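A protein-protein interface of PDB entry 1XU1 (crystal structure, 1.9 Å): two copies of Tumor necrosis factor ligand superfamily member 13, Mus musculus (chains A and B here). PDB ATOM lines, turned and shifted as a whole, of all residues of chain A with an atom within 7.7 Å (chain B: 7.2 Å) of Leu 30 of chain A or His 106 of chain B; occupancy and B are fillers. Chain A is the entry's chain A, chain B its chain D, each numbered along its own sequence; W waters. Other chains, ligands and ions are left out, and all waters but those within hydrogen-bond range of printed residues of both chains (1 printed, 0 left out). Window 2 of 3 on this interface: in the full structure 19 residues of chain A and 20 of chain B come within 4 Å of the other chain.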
ATOM      1  N   VAL A   5     -18.238  27.717  -0.253  1.00  0.00           N
ATOM      2  CA  VAL A   5     -18.633  26.320  -0.313  1.00  0.00           C
ATOM      3  C   VAL A   5     -18.626  25.777  -1.744  1.00  0.00           C
ATOM      4  O   VAL A   5     -18.860  26.514  -2.712  1.00  0.00           O
ATOM      5  CB  VAL A   5     -20.028  26.044   0.344  1.00  0.00           C
ATOM      6  CG1 VAL A   5     -20.164  26.737   1.709  1.00  0.00           C
ATOM      7  CG2 VAL A   5     -21.154  26.400  -0.561  1.00  0.00           C
ATOM      8  N   LEU A   6     -18.377  24.479  -1.854  1.00  0.00           N
ATOM      9  CA  LEU A   6     -18.392  23.775  -3.128  1.00  0.00           C
ATOM     10  C   LEU A   6     -18.843  22.343  -2.895  1.00  0.00           C
ATOM     11  O   LEU A   6     -18.177  21.606  -2.191  1.00  0.00           O
ATOM     12  CB  LEU A   6     -17.006  23.799  -3.785  1.00  0.00           C
ATOM     13  CG  LEU A   6     -16.965  23.253  -5.212  1.00  0.00           C
ATOM     14  CD1 LEU A   6     -17.761  24.137  -6.170  1.00  0.00           C
ATOM     15  CD2 LEU A   6     -15.515  23.104  -5.687  1.00  0.00           C
ATOM     16  N   HIS A   7     -19.971  21.951  -3.483  1.00  0.00           N
ATOM     17  CA  HIS A   7     -20.451  20.565  -3.380  1.00  0.00           C
ATOM     18  C   HIS A   7     -20.477  19.996  -4.792  1.00  0.00           C
ATOM     19  O   HIS A   7     -21.044  20.594  -5.686  1.00  0.00           O
ATOM     20  CB  HIS A   7     -21.828  20.511  -2.716  1.00  0.00           C
ATOM     21  CG  HIS A   7     -22.363  19.126  -2.497  1.00  0.00           C
ATOM     22  ND1 HIS A   7     -21.981  18.338  -1.431  1.00  0.00           N
ATOM     23  CD2 HIS A   7     -23.317  18.424  -3.156  1.00  0.00           C
ATOM     24  CE1 HIS A   7     -22.634  17.187  -1.479  1.00  0.00           C
ATOM     25  NE2 HIS A   7     -23.460  17.218  -2.512  1.00  0.00           N
ATOM     26  N   LEU A   8     -19.844  18.838  -4.970  1.00  0.00           N
ATOM     27  CA  LEU A   8     -19.614  18.234  -6.277  1.00  0.00           C
ATOM     28  C   LEU A   8     -20.253  16.862  -6.319  1.00  0.00           C
ATOM     29  O   LEU A   8     -20.234  16.131  -5.319  1.00  0.00           O
ATOM     30  CB  LEU A   8     -18.124  18.071  -6.567  1.00  0.00           C
ATOM     31  CG  LEU A   8     -17.232  19.326  -6.551  1.00  0.00           C
ATOM     32  CD1 LEU A   8     -15.764  18.917  -6.637  1.00  0.00           C
ATOM     33  CD2 LEU A   8     -17.560  20.264  -7.667  1.00  0.00           C
ATOM     34  N   VAL A   9     -20.794  16.523  -7.485  1.00  0.00           N
ATOM     35  CA  VAL A   9     -21.352  15.193  -7.753  1.00  0.00           C
ATOM     36  C   VAL A   9     -20.759  14.630  -9.056  1.00  0.00           C
ATOM     37  O   VAL A   9     -20.187  15.378  -9.861  1.00  0.00           O
ATOM     38  CB  VAL A   9     -22.904  15.222  -7.831  1.00  0.00           C
ATOM     39  CG1 VAL A   9     -23.501  15.784  -6.523  1.00  0.00           C
ATOM     40  CG2 VAL A   9     -23.380  16.014  -9.043  1.00  0.00           C
ATOM     41  N   GLN A  27     -18.768  17.506 -11.225  1.00  0.00           N
ATOM     42  CA  GLN A  27     -19.452  18.720 -11.662  1.00  0.00           C
ATOM     43  C   GLN A  27     -20.024  19.411 -10.425  1.00  0.00           C
ATOM     44  O   GLN A  27     -20.565  18.743  -9.549  1.00  0.00           O
ATOM     45  CB  GLN A  27     -20.594  18.399 -12.646  1.00  0.00           C
ATOM     46  CG  GLN A  27     -21.605  17.357 -12.143  1.00  0.00           C
ATOM     47  CD  GLN A  27     -22.840  17.192 -13.039  1.00  0.00           C
ATOM     48  OE1 GLN A  27     -23.233  18.114 -13.750  1.00  0.00           O
ATOM     49  NE2 GLN A  27     -23.450  16.008 -12.991  1.00  0.00           N
ATOM     50  N   PRO A  28     -19.917  20.736 -10.350  1.00  0.00           N
ATOM     51  CA  PRO A  28     -20.492  21.490  -9.230  1.00  0.00           C
ATOM     52  C   PRO A  28     -22.016  21.513  -9.235  1.00  0.00           C
ATOM     53  O   PRO A  28     -22.611  21.702 -10.284  1.00  0.00           O
ATOM     54  CB  PRO A  28     -19.940  22.905  -9.437  1.00  0.00           C
ATOM     55  CG  PRO A  28     -19.602  22.996 -10.865  1.00  0.00           C
ATOM     56  CD  PRO A  28     -19.205  21.607 -11.307  1.00  0.00           C
ATOM     57  N   VAL A  29     -22.634  21.332  -8.073  1.00  0.00           N
ATOM     58  CA  VAL A  29     -24.080  21.562  -7.926  1.00  0.00           C
ATOM     59  C   VAL A  29     -24.419  22.664  -6.907  1.00  0.00           C
ATOM     60  O   VAL A  29     -25.553  23.146  -6.860  1.00  0.00           O
ATOM     61  CB  VAL A  29     -24.856  20.261  -7.602  1.00  0.00           C
ATOM     62  CG1 VAL A  29     -24.774  19.298  -8.776  1.00  0.00           C
ATOM     63  CG2 VAL A  29     -24.348  19.596  -6.335  1.00  0.00           C
ATOM     64  N   LEU A  30     -23.439  23.064  -6.104  1.00  0.00           N
ATOM     65  CA  LEU A  30     -23.597  24.186  -5.181  1.00  0.00           C
ATOM     66  C   LEU A  30     -22.264  24.907  -5.083  1.00  0.00           C
ATOM     67  O   LEU A  30     -21.236  24.293  -4.846  1.00  0.00           O
ATOM     68  CB  LEU A  30     -24.059  23.709  -3.790  1.00  0.00           C
ATOM     69  CG  LEU A  30     -24.272  24.777  -2.702  1.00  0.00           C
ATOM     70  CD1 LEU A  30     -25.263  25.840  -3.133  1.00  0.00           C
ATOM     71  CD2 LEU A  30     -24.712  24.142  -1.381  1.00  0.00           C
ATOM     72  N   ARG A  31     -22.290  26.216  -5.265  1.00  0.00           N
ATOM     73  CA  ARG A  31     -21.083  27.031  -5.215  1.00  0.00           C
ATOM     74  C   ARG A  31     -21.401  28.400  -4.631  1.00  0.00           C
ATOM     75  O   ARG A  31     -22.346  29.058  -5.057  1.00  0.00           O
ATOM     76  CB  ARG A  31     -20.502  27.198  -6.630  1.00  0.00           C
ATOM     77  CG  ARG A  31     -19.137  27.898  -6.684  1.00  0.00           C
ATOM     78  CD  ARG A  31     -18.794  28.472  -8.056  1.00  0.00           C
ATOM     79  NE  ARG A  31     -18.944  27.469  -9.117  1.00  0.00           N
ATOM     80  CZ  ARG A  31     -19.296  27.725 -10.384  1.00  0.00           C
ATOM     81  NH1 ARG A  31     -19.544  28.970 -10.797  1.00  0.00           N
ATOM     82  NH2 ARG A  31     -19.401  26.723 -11.253  1.00  0.00           N
ATOM     83  N   ARG A  32     -20.606  28.808  -3.649  1.00  0.00           N
ATOM     84  CA  ARG A  32     -20.580  30.174  -3.147  1.00  0.00           C
ATOM     85  C   ARG A  32     -19.116  30.563  -2.939  1.00  0.00           C
ATOM     86  O   ARG A  32     -18.344  29.785  -2.389  1.00  0.00           O
ATOM     87  CB  ARG A  32     -21.359  30.263  -1.831  1.00  0.00           C
ATOM     88  CG  ARG A  32     -21.450  31.665  -1.240  1.00  0.00           C
ATOM     89  CD  ARG A  32     -22.401  31.773  -0.058  1.00  0.00           C
ATOM     90  NE  ARG A  32     -21.874  31.105   1.128  1.00  0.00           N
ATOM     91  CZ  ARG A  32     -22.569  30.901   2.245  1.00  0.00           C
ATOM     92  NH1 ARG A  32     -23.833  31.311   2.343  1.00  0.00           N
ATOM     93  NH2 ARG A  32     -22.001  30.283   3.272  1.00  0.00           N
ATOM     94  N   TYR A  54     -14.959  16.878   2.748  1.00  0.00           N
ATOM     95  CA  TYR A  54     -15.723  15.642   2.983  1.00  0.00           C
ATOM     96  C   TYR A  54     -15.926  14.882   1.677  1.00  0.00           C
ATOM     97  O   TYR A  54     -16.024  15.479   0.589  1.00  0.00           O
ATOM     98  CB  TYR A  54     -17.081  15.902   3.661  1.00  0.00           C
ATOM     99  CG  TYR A  54     -18.045  16.793   2.890  1.00  0.00           C
ATOM    100  CD1 TYR A  54     -18.035  18.164   3.059  1.00  0.00           C
ATOM    101  CD2 TYR A  54     -18.995  16.246   2.030  1.00  0.00           C
ATOM    102  CE1 TYR A  54     -18.930  18.978   2.367  1.00  0.00           C
ATOM    103  CE2 TYR A  54     -19.889  17.041   1.349  1.00  0.00           C
ATOM    104  CZ  TYR A  54     -19.849  18.408   1.512  1.00  0.00           C
ATOM    105  OH  TYR A  54     -20.741  19.198   0.829  1.00  0.00           O
ATOM    106  N   LEU A 133     -18.515  14.971  -3.140  1.00  0.00           N
ATOM    107  CA  LEU A 133     -17.294  15.564  -2.621  1.00  0.00           C
ATOM    108  C   LEU A 133     -17.594  17.025  -2.346  1.00  0.00           C
ATOM    109  O   LEU A 133     -18.220  17.680  -3.158  1.00  0.00           O
ATOM    110  CB  LEU A 133     -16.169  15.455  -3.656  1.00  0.00           C
ATOM    111  CG  LEU A 133     -14.813  16.131  -3.394  1.00  0.00           C
ATOM    112  CD1 LEU A 133     -14.112  15.475  -2.245  1.00  0.00           C
ATOM    113  CD2 LEU A 133     -13.916  16.085  -4.657  1.00  0.00           C
ATOM    114  N   GLY A 134     -17.161  17.542  -1.205  1.00  0.00           N
ATOM    115  CA  GLY A 134     -17.386  18.945  -0.912  1.00  0.00           C
ATOM    116  C   GLY A 134     -16.353  19.587  -0.012  1.00  0.00           C
ATOM    117  O   GLY A 134     -15.532  18.921   0.649  1.00  0.00           O
ATOM    118  N   PHE A 135     -16.442  20.910   0.032  1.00  0.00           N
ATOM    119  CA  PHE A 135     -15.442  21.765   0.657  1.00  0.00           C
ATOM    120  C   PHE A 135     -16.163  22.940   1.299  1.00  0.00           C
ATOM    121  O   PHE A 135     -17.081  23.510   0.704  1.00  0.00           O
ATOM    122  CB  PHE A 135     -14.497  22.362  -0.391  1.00  0.00           C
ATOM    123  CG  PHE A 135     -13.723  21.350  -1.203  1.00  0.00           C
ATOM    124  CD1 PHE A 135     -14.307  20.703  -2.277  1.00  0.00           C
ATOM    125  CD2 PHE A 135     -12.391  21.101  -0.931  1.00  0.00           C
ATOM    126  CE1 PHE A 135     -13.600  19.792  -3.031  1.00  0.00           C
ATOM    127  CE2 PHE A 135     -11.672  20.190  -1.694  1.00  0.00           C
ATOM    128  CZ  PHE A 135     -12.278  19.533  -2.740  1.00  0.00           C
ATOM    129  N   THR B  48     -34.247  30.379   4.552  1.00  0.00           N
ATOM    130  CA  THR B  48     -33.434  29.989   3.397  1.00  0.00           C
ATOM    131  C   THR B  48     -31.944  30.184   3.682  1.00  0.00           C
ATOM    132  O   THR B  48     -31.538  31.183   4.277  1.00  0.00           O
ATOM    133  CB  THR B  48     -33.821  30.823   2.157  1.00  0.00           C
ATOM    134  OG1 THR B  48     -35.177  30.558   1.790  1.00  0.00           O
ATOM    135  CG2 THR B  48     -33.015  30.402   0.920  1.00  0.00           C
ATOM    136  N   GLY B  49     -31.128  29.230   3.257  1.00  0.00           N
ATOM    137  CA  GLY B  49     -29.688  29.365   3.391  1.00  0.00           C
ATOM    138  C   GLY B  49     -28.933  28.101   3.042  1.00  0.00           C
ATOM    139  O   GLY B  49     -29.526  27.105   2.632  1.00  0.00           O
ATOM    140  N   ILE B  50     -27.617  28.147   3.218  1.00  0.00           N
ATOM    141  CA  ILE B  50     -26.770  26.980   3.039  1.00  0.00           C
ATOM    142  C   ILE B  50     -26.515  26.349   4.411  1.00  0.00           C
ATOM    143  O   ILE B  50     -26.119  27.030   5.340  1.00  0.00           O
ATOM    144  CB  ILE B  50     -25.452  27.367   2.340  1.00  0.00           C
ATOM    145  CG1 ILE B  50     -25.747  27.867   0.917  1.00  0.00           C
ATOM    146  CG2 ILE B  50     -24.534  26.166   2.251  1.00  0.00           C
ATOM    147  CD1 ILE B  50     -24.556  28.444   0.207  1.00  0.00           C
ATOM    148  N   TYR B  51     -26.776  25.056   4.533  1.00  0.00           N
ATOM    149  CA  TYR B  51     -26.635  24.352   5.796  1.00  0.00           C
ATOM    150  C   TYR B  51     -25.772  23.133   5.631  1.00  0.00           C
ATOM    151  O   TYR B  51     -25.908  22.409   4.649  1.00  0.00           O
ATOM    152  CB  TYR B  51     -27.989  23.857   6.286  1.00  0.00           C
ATOM    153  CG  TYR B  51     -28.983  24.924   6.675  1.00  0.00           C
ATOM    154  CD1 TYR B  51     -29.754  25.585   5.713  1.00  0.00           C
ATOM    155  CD2 TYR B  51     -29.189  25.237   8.014  1.00  0.00           C
ATOM    156  CE1 TYR B  51     -30.698  26.563   6.108  1.00  0.00           C
ATOM    157  CE2 TYR B  51     -30.118  26.177   8.405  1.00  0.00           C
ATOM    158  CZ  TYR B  51     -30.871  26.833   7.461  1.00  0.00           C
ATOM    159  OH  TYR B  51     -31.776  27.765   7.885  1.00  0.00           O
ATOM    160  N   ARG B  72     -35.162  16.400   0.835  1.00  0.00           N
ATOM    161  CA  ARG B  72     -35.774  17.714   0.957  1.00  0.00           C
ATOM    162  C   ARG B  72     -37.052  17.699   0.114  1.00  0.00           C
ATOM    163  O   ARG B  72     -37.030  17.285  -1.039  1.00  0.00           O
ATOM    164  CB  ARG B  72     -34.795  18.754   0.419  1.00  0.00           C
ATOM    165  CG  ARG B  72     -35.295  20.165   0.272  1.00  0.00           C
ATOM    166  CD  ARG B  72     -34.258  21.069  -0.405  1.00  0.00           C
ATOM    167  NE  ARG B  72     -34.191  20.852  -1.844  1.00  0.00           N
ATOM    168  CZ  ARG B  72     -35.084  21.301  -2.724  1.00  0.00           C
ATOM    169  NH1 ARG B  72     -36.137  22.016  -2.334  1.00  0.00           N
ATOM    170  NH2 ARG B  72     -34.923  21.038  -4.016  1.00  0.00           N
ATOM    171  N   GLU B  79     -36.414  15.748  -3.480  1.00  0.00           N
ATOM    172  CA  GLU B  79     -35.024  15.587  -3.891  1.00  0.00           C
ATOM    173  C   GLU B  79     -34.250  14.869  -2.785  1.00  0.00           C
ATOM    174  O   GLU B  79     -34.273  15.298  -1.631  1.00  0.00           O
ATOM    175  CB  GLU B  79     -34.404  16.956  -4.171  1.00  0.00           C
ATOM    176  CG  GLU B  79     -32.888  16.957  -4.272  1.00  0.00           C
ATOM    177  CD  GLU B  79     -32.333  18.245  -4.833  1.00  0.00           C
ATOM    178  OE1 GLU B  79     -32.150  18.315  -6.072  1.00  0.00           O
ATOM    179  OE2 GLU B  79     -32.075  19.180  -4.032  1.00  0.00           O
ATOM    180  N   LEU B  81     -31.008  14.195  -0.821  1.00  0.00           N
ATOM    181  CA  LEU B  81     -29.749  14.882  -0.575  1.00  0.00           C
ATOM    182  C   LEU B  81     -28.596  13.896  -0.447  1.00  0.00           C
ATOM    183  O   LEU B  81     -27.585  14.039  -1.140  1.00  0.00           O
ATOM    184  CB  LEU B  81     -29.852  15.770   0.656  1.00  0.00           C
ATOM    185  CG  LEU B  81     -31.013  16.765   0.603  1.00  0.00           C
ATOM    186  CD1 LEU B  81     -31.047  17.561   1.887  1.00  0.00           C
ATOM    187  CD2 LEU B  81     -30.905  17.670  -0.620  1.00  0.00           C
ATOM    188  N   VAL B 104     -23.328  19.541   2.509  1.00  0.00           N
ATOM    189  CA  VAL B 104     -23.716  20.943   2.570  1.00  0.00           C
ATOM    190  C   VAL B 104     -24.718  21.211   1.441  1.00  0.00           C
ATOM    191  O   VAL B 104     -24.461  20.888   0.273  1.00  0.00           O
ATOM    192  CB  VAL B 104     -22.483  21.857   2.488  1.00  0.00           C
ATOM    193  CG1 VAL B 104     -22.889  23.318   2.386  1.00  0.00           C
ATOM    194  CG2 VAL B 104     -21.578  21.631   3.715  1.00  0.00           C
ATOM    195  N   PHE B 105     -25.865  21.788   1.795  1.00  0.00           N
ATOM    196  CA  PHE B 105     -27.004  21.922   0.875  1.00  0.00           C
ATOM    197  C   PHE B 105     -27.723  23.256   0.997  1.00  0.00           C
ATOM    198  O   PHE B 105     -27.819  23.826   2.087  1.00  0.00           O
ATOM    199  CB  PHE B 105     -28.000  20.781   1.127  1.00  0.00           C
ATOM    200  CG  PHE B 105     -27.390  19.426   1.002  1.00  0.00           C
ATOM    201  CD1 PHE B 105     -27.201  18.860  -0.250  1.00  0.00           C
ATOM    202  CD2 PHE B 105     -26.947  18.737   2.124  1.00  0.00           C
ATOM    203  CE1 PHE B 105     -26.595  17.610  -0.377  1.00  0.00           C
ATOM    204  CE2 PHE B 105     -26.350  17.480   1.995  1.00  0.00           C
ATOM    205  CZ  PHE B 105     -26.170  16.937   0.745  1.00  0.00           C
ATOM    206  N   HIS B 106     -28.231  23.764  -0.130  1.00  0.00           N
ATOM    207  CA  HIS B 106     -29.072  24.949  -0.113  1.00  0.00           C
ATOM    208  C   HIS B 106     -30.498  24.536   0.209  1.00  0.00           C
ATOM    209  O   HIS B 106     -31.107  23.759  -0.540  1.00  0.00           O
ATOM    210  CB  HIS B 106     -29.045  25.692  -1.437  1.00  0.00           C
ATOM    211  CG  HIS B 106     -29.706  27.031  -1.373  1.00  0.00           C
ATOM    212  ND1 HIS B 106     -29.041  28.170  -0.973  1.00  0.00           N
ATOM    213  CD2 HIS B 106     -30.982  27.408  -1.610  1.00  0.00           C
ATOM    214  CE1 HIS B 106     -29.872  29.197  -1.002  1.00  0.00           C
ATOM    215  NE2 HIS B 106     -31.057  28.761  -1.387  1.00  0.00           N
ATOM    216  N   LEU B 107     -31.004  25.022   1.341  1.00  0.00           N
ATOM    217  CA  LEU B 107     -32.361  24.711   1.804  1.00  0.00           C
ATOM    218  C   LEU B 107     -33.199  25.982   1.742  1.00  0.00           C
ATOM    219  O   LEU B 107     -32.732  27.065   2.096  1.00  0.00           O
ATOM    220  CB  LEU B 107     -32.354  24.154   3.232  1.00  0.00           C
ATOM    221  CG  LEU B 107     -31.503  22.913   3.513  1.00  0.00           C
ATOM    222  CD1 LEU B 107     -31.691  22.459   4.943  1.00  0.00           C
ATOM    223  CD2 LEU B 107     -31.818  21.759   2.544  1.00  0.00           C
ATOM    224  N   HIS B 108     -34.428  25.851   1.255  1.00  0.00           N
ATOM    225  CA  HIS B 108     -35.331  26.990   1.087  1.00  0.00           C
ATOM    226  C   HIS B 108     -36.390  27.025   2.191  1.00  0.00           C
ATOM    227  O   HIS B 108     -36.825  25.986   2.682  1.00  0.00           O
ATOM    228  CB  HIS B 108     -36.046  26.902  -0.261  1.00  0.00           C
ATOM    229  CG  HIS B 108     -35.134  27.012  -1.443  1.00  0.00           C
ATOM    230  ND1 HIS B 108     -34.946  28.192  -2.132  1.00  0.00           N
ATOM    231  CD2 HIS B 108     -34.363  26.087  -2.064  1.00  0.00           C
ATOM    232  CE1 HIS B 108     -34.099  27.990  -3.126  1.00  0.00           C
ATOM    233  NE2 HIS B 108     -33.732  26.720  -3.106  1.00  0.00           N
ATOM    234  N   GLN B 109     -36.803  28.229   2.552  1.00  0.00           N
ATOM    235  CA  GLN B 109     -37.980  28.470   3.385  1.00  0.00           C
ATOM    236  C   GLN B 109     -39.173  27.637   2.899  1.00  0.00           C
ATOM    237  O   GLN B 109     -39.514  27.670   1.709  1.00  0.00           O
ATOM    238  CB  GLN B 109     -38.315  29.959   3.317  1.00  0.00           C
ATOM    239  CG  GLN B 109     -39.544  30.413   4.058  1.00  0.00           C
ATOM    240  CD  GLN B 109     -39.673  31.931   4.032  1.00  0.00           C
ATOM    241  OE1 GLN B 109     -40.344  32.484   3.161  1.00  0.00           O
ATOM    242  NE2 GLN B 109     -39.011  32.602   4.969  1.00  0.00           N
ATOM    243  N   ASP B 111     -39.269  24.298   3.031  1.00  0.00           N
ATOM    244  CA  ASP B 111     -38.808  22.939   2.798  1.00  0.00           C
ATOM    245  C   ASP B 111     -39.072  22.067   4.020  1.00  0.00           C
ATOM    246  O   ASP B 111     -39.096  22.548   5.137  1.00  0.00           O
ATOM    247  CB  ASP B 111     -37.307  22.903   2.519  1.00  0.00           C
ATOM    248  CG  ASP B 111     -36.953  23.307   1.105  1.00  0.00           C
ATOM    249  OD1 ASP B 111     -37.850  23.629   0.289  1.00  0.00           O
ATOM    250  OD2 ASP B 111     -35.765  23.326   0.721  1.00  0.00           O
HETATM  251  O   HOH W   1     -25.453  15.100  -2.879  1.00  0.00           O
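The side-chain hydroxyl of Tyr 54 of chain A sits at hydrogen-bond distance from the backbone NH of Val 104 of chain B (3.1 Å).
O of Tyr 51 of chain B lies within hydrogen-bond range of N of Phe 105 of chain B, 2.9 Å away. The backbone carbonyl oxygen (O) of His 7 of chain A lies within hydrogen-bond range of the backbone NH (N) of Val 29 of chain A. The backbone carbonyl oxygen (O) of Tyr 54 of chain A sits at hydrogen-bond distance from the backbone NH (N) of Gly 134 of chain A, at 3.0 Å. The backbone NH of Val 5 of chain A sits at hydrogen-bond distance from the backbone carbonyl oxygen of Arg 32 of chain A (3.0 Å). ND1 of His 7 of chain A is in hydrogen-bond range of OH of Tyr 54 of chain A (2.7 Å). N of His 7 of chain A is in hydrogen-bond range of O of Leu 30 of chain A, at 3.0 Å.
Among the printed residues, pairs that only touch across the chains: Arg 32 of chain A with Ile 50 of chain B, Leu 30 of chain A with Val 104 of chain B, Leu 30 of chain A with His 106 of chain B, His 7 of chain A with Phe 105 of chain B, His 7 of chain A with Val 104 of chain B and Leu 30 of chain A with Phe 105 of chain B.
Of the printed residues of chain B, His 7 of chain A touches Val 104 (3.9 Å) and Phe 105 (3.8 Å). Of chain B, only Val 104, Phe 105 and His 106 come within 4 Å of Leu 30 of chain A. Arg 31 of chain A touches none of the printed residues of chain B. Printed residues of chain B within 4 Å of Arg 32 of chain A: Ile 50. Gly 134 of chain A touches none of the printed residues of chain B. Of the printed residues of chain A, Ile 50 of chain B touches Arg 32 (3.6 Å). Printed residues of chain A within 4 Å of Val 104 of chain B: His 7, Leu 30 and Tyr 54. Printed residues of chain A within 4 Å of Phe 105 of chain B: His 7 and Leu 30. Printed residues of chain A within 4 Å of His 106 of chain B: Leu 30. The nearest residue of chain B that does not touch Leu 30 of chain A is Ile 50 of chain B (4.2 Å). The nearest printed residue of chain A that does not touch His 106 of chain B is Arg 32 of chain A (6.9 Å).
Of the 14 printed residues of chain B, 4 touch a printed residue of chain A. Printed residues of chain B that touch a printed residue of chain A: Ile 50, Val 104, Phe 105 and His 106. Along chain B the printed residues that touch a printed residue of chain A span positions 50 to 106. Hydrophobic or aromatic side chains of chain A that line the printed part of chain B: His 7, Leu 30 and Tyr 54. Among the printed residues, 7 pairs touch across the chains. Among the printed residues, no Asp or Glu carboxylate lies within 4 Å of a Lys or Arg side-chain nitrogen of the other chain.
No position is printed for both chains. Of the 7 pairs that touch across the chains among the printed residues, none has its exchanged pair printed and touching as well.
Water W1 lies within hydrogen-bond range of a ring nitrogen (NE2) of His 7 of chain A (2.9 Å) and the backbone carbonyl oxygen (O) of Leu 81 of chain B (2.9 Å).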
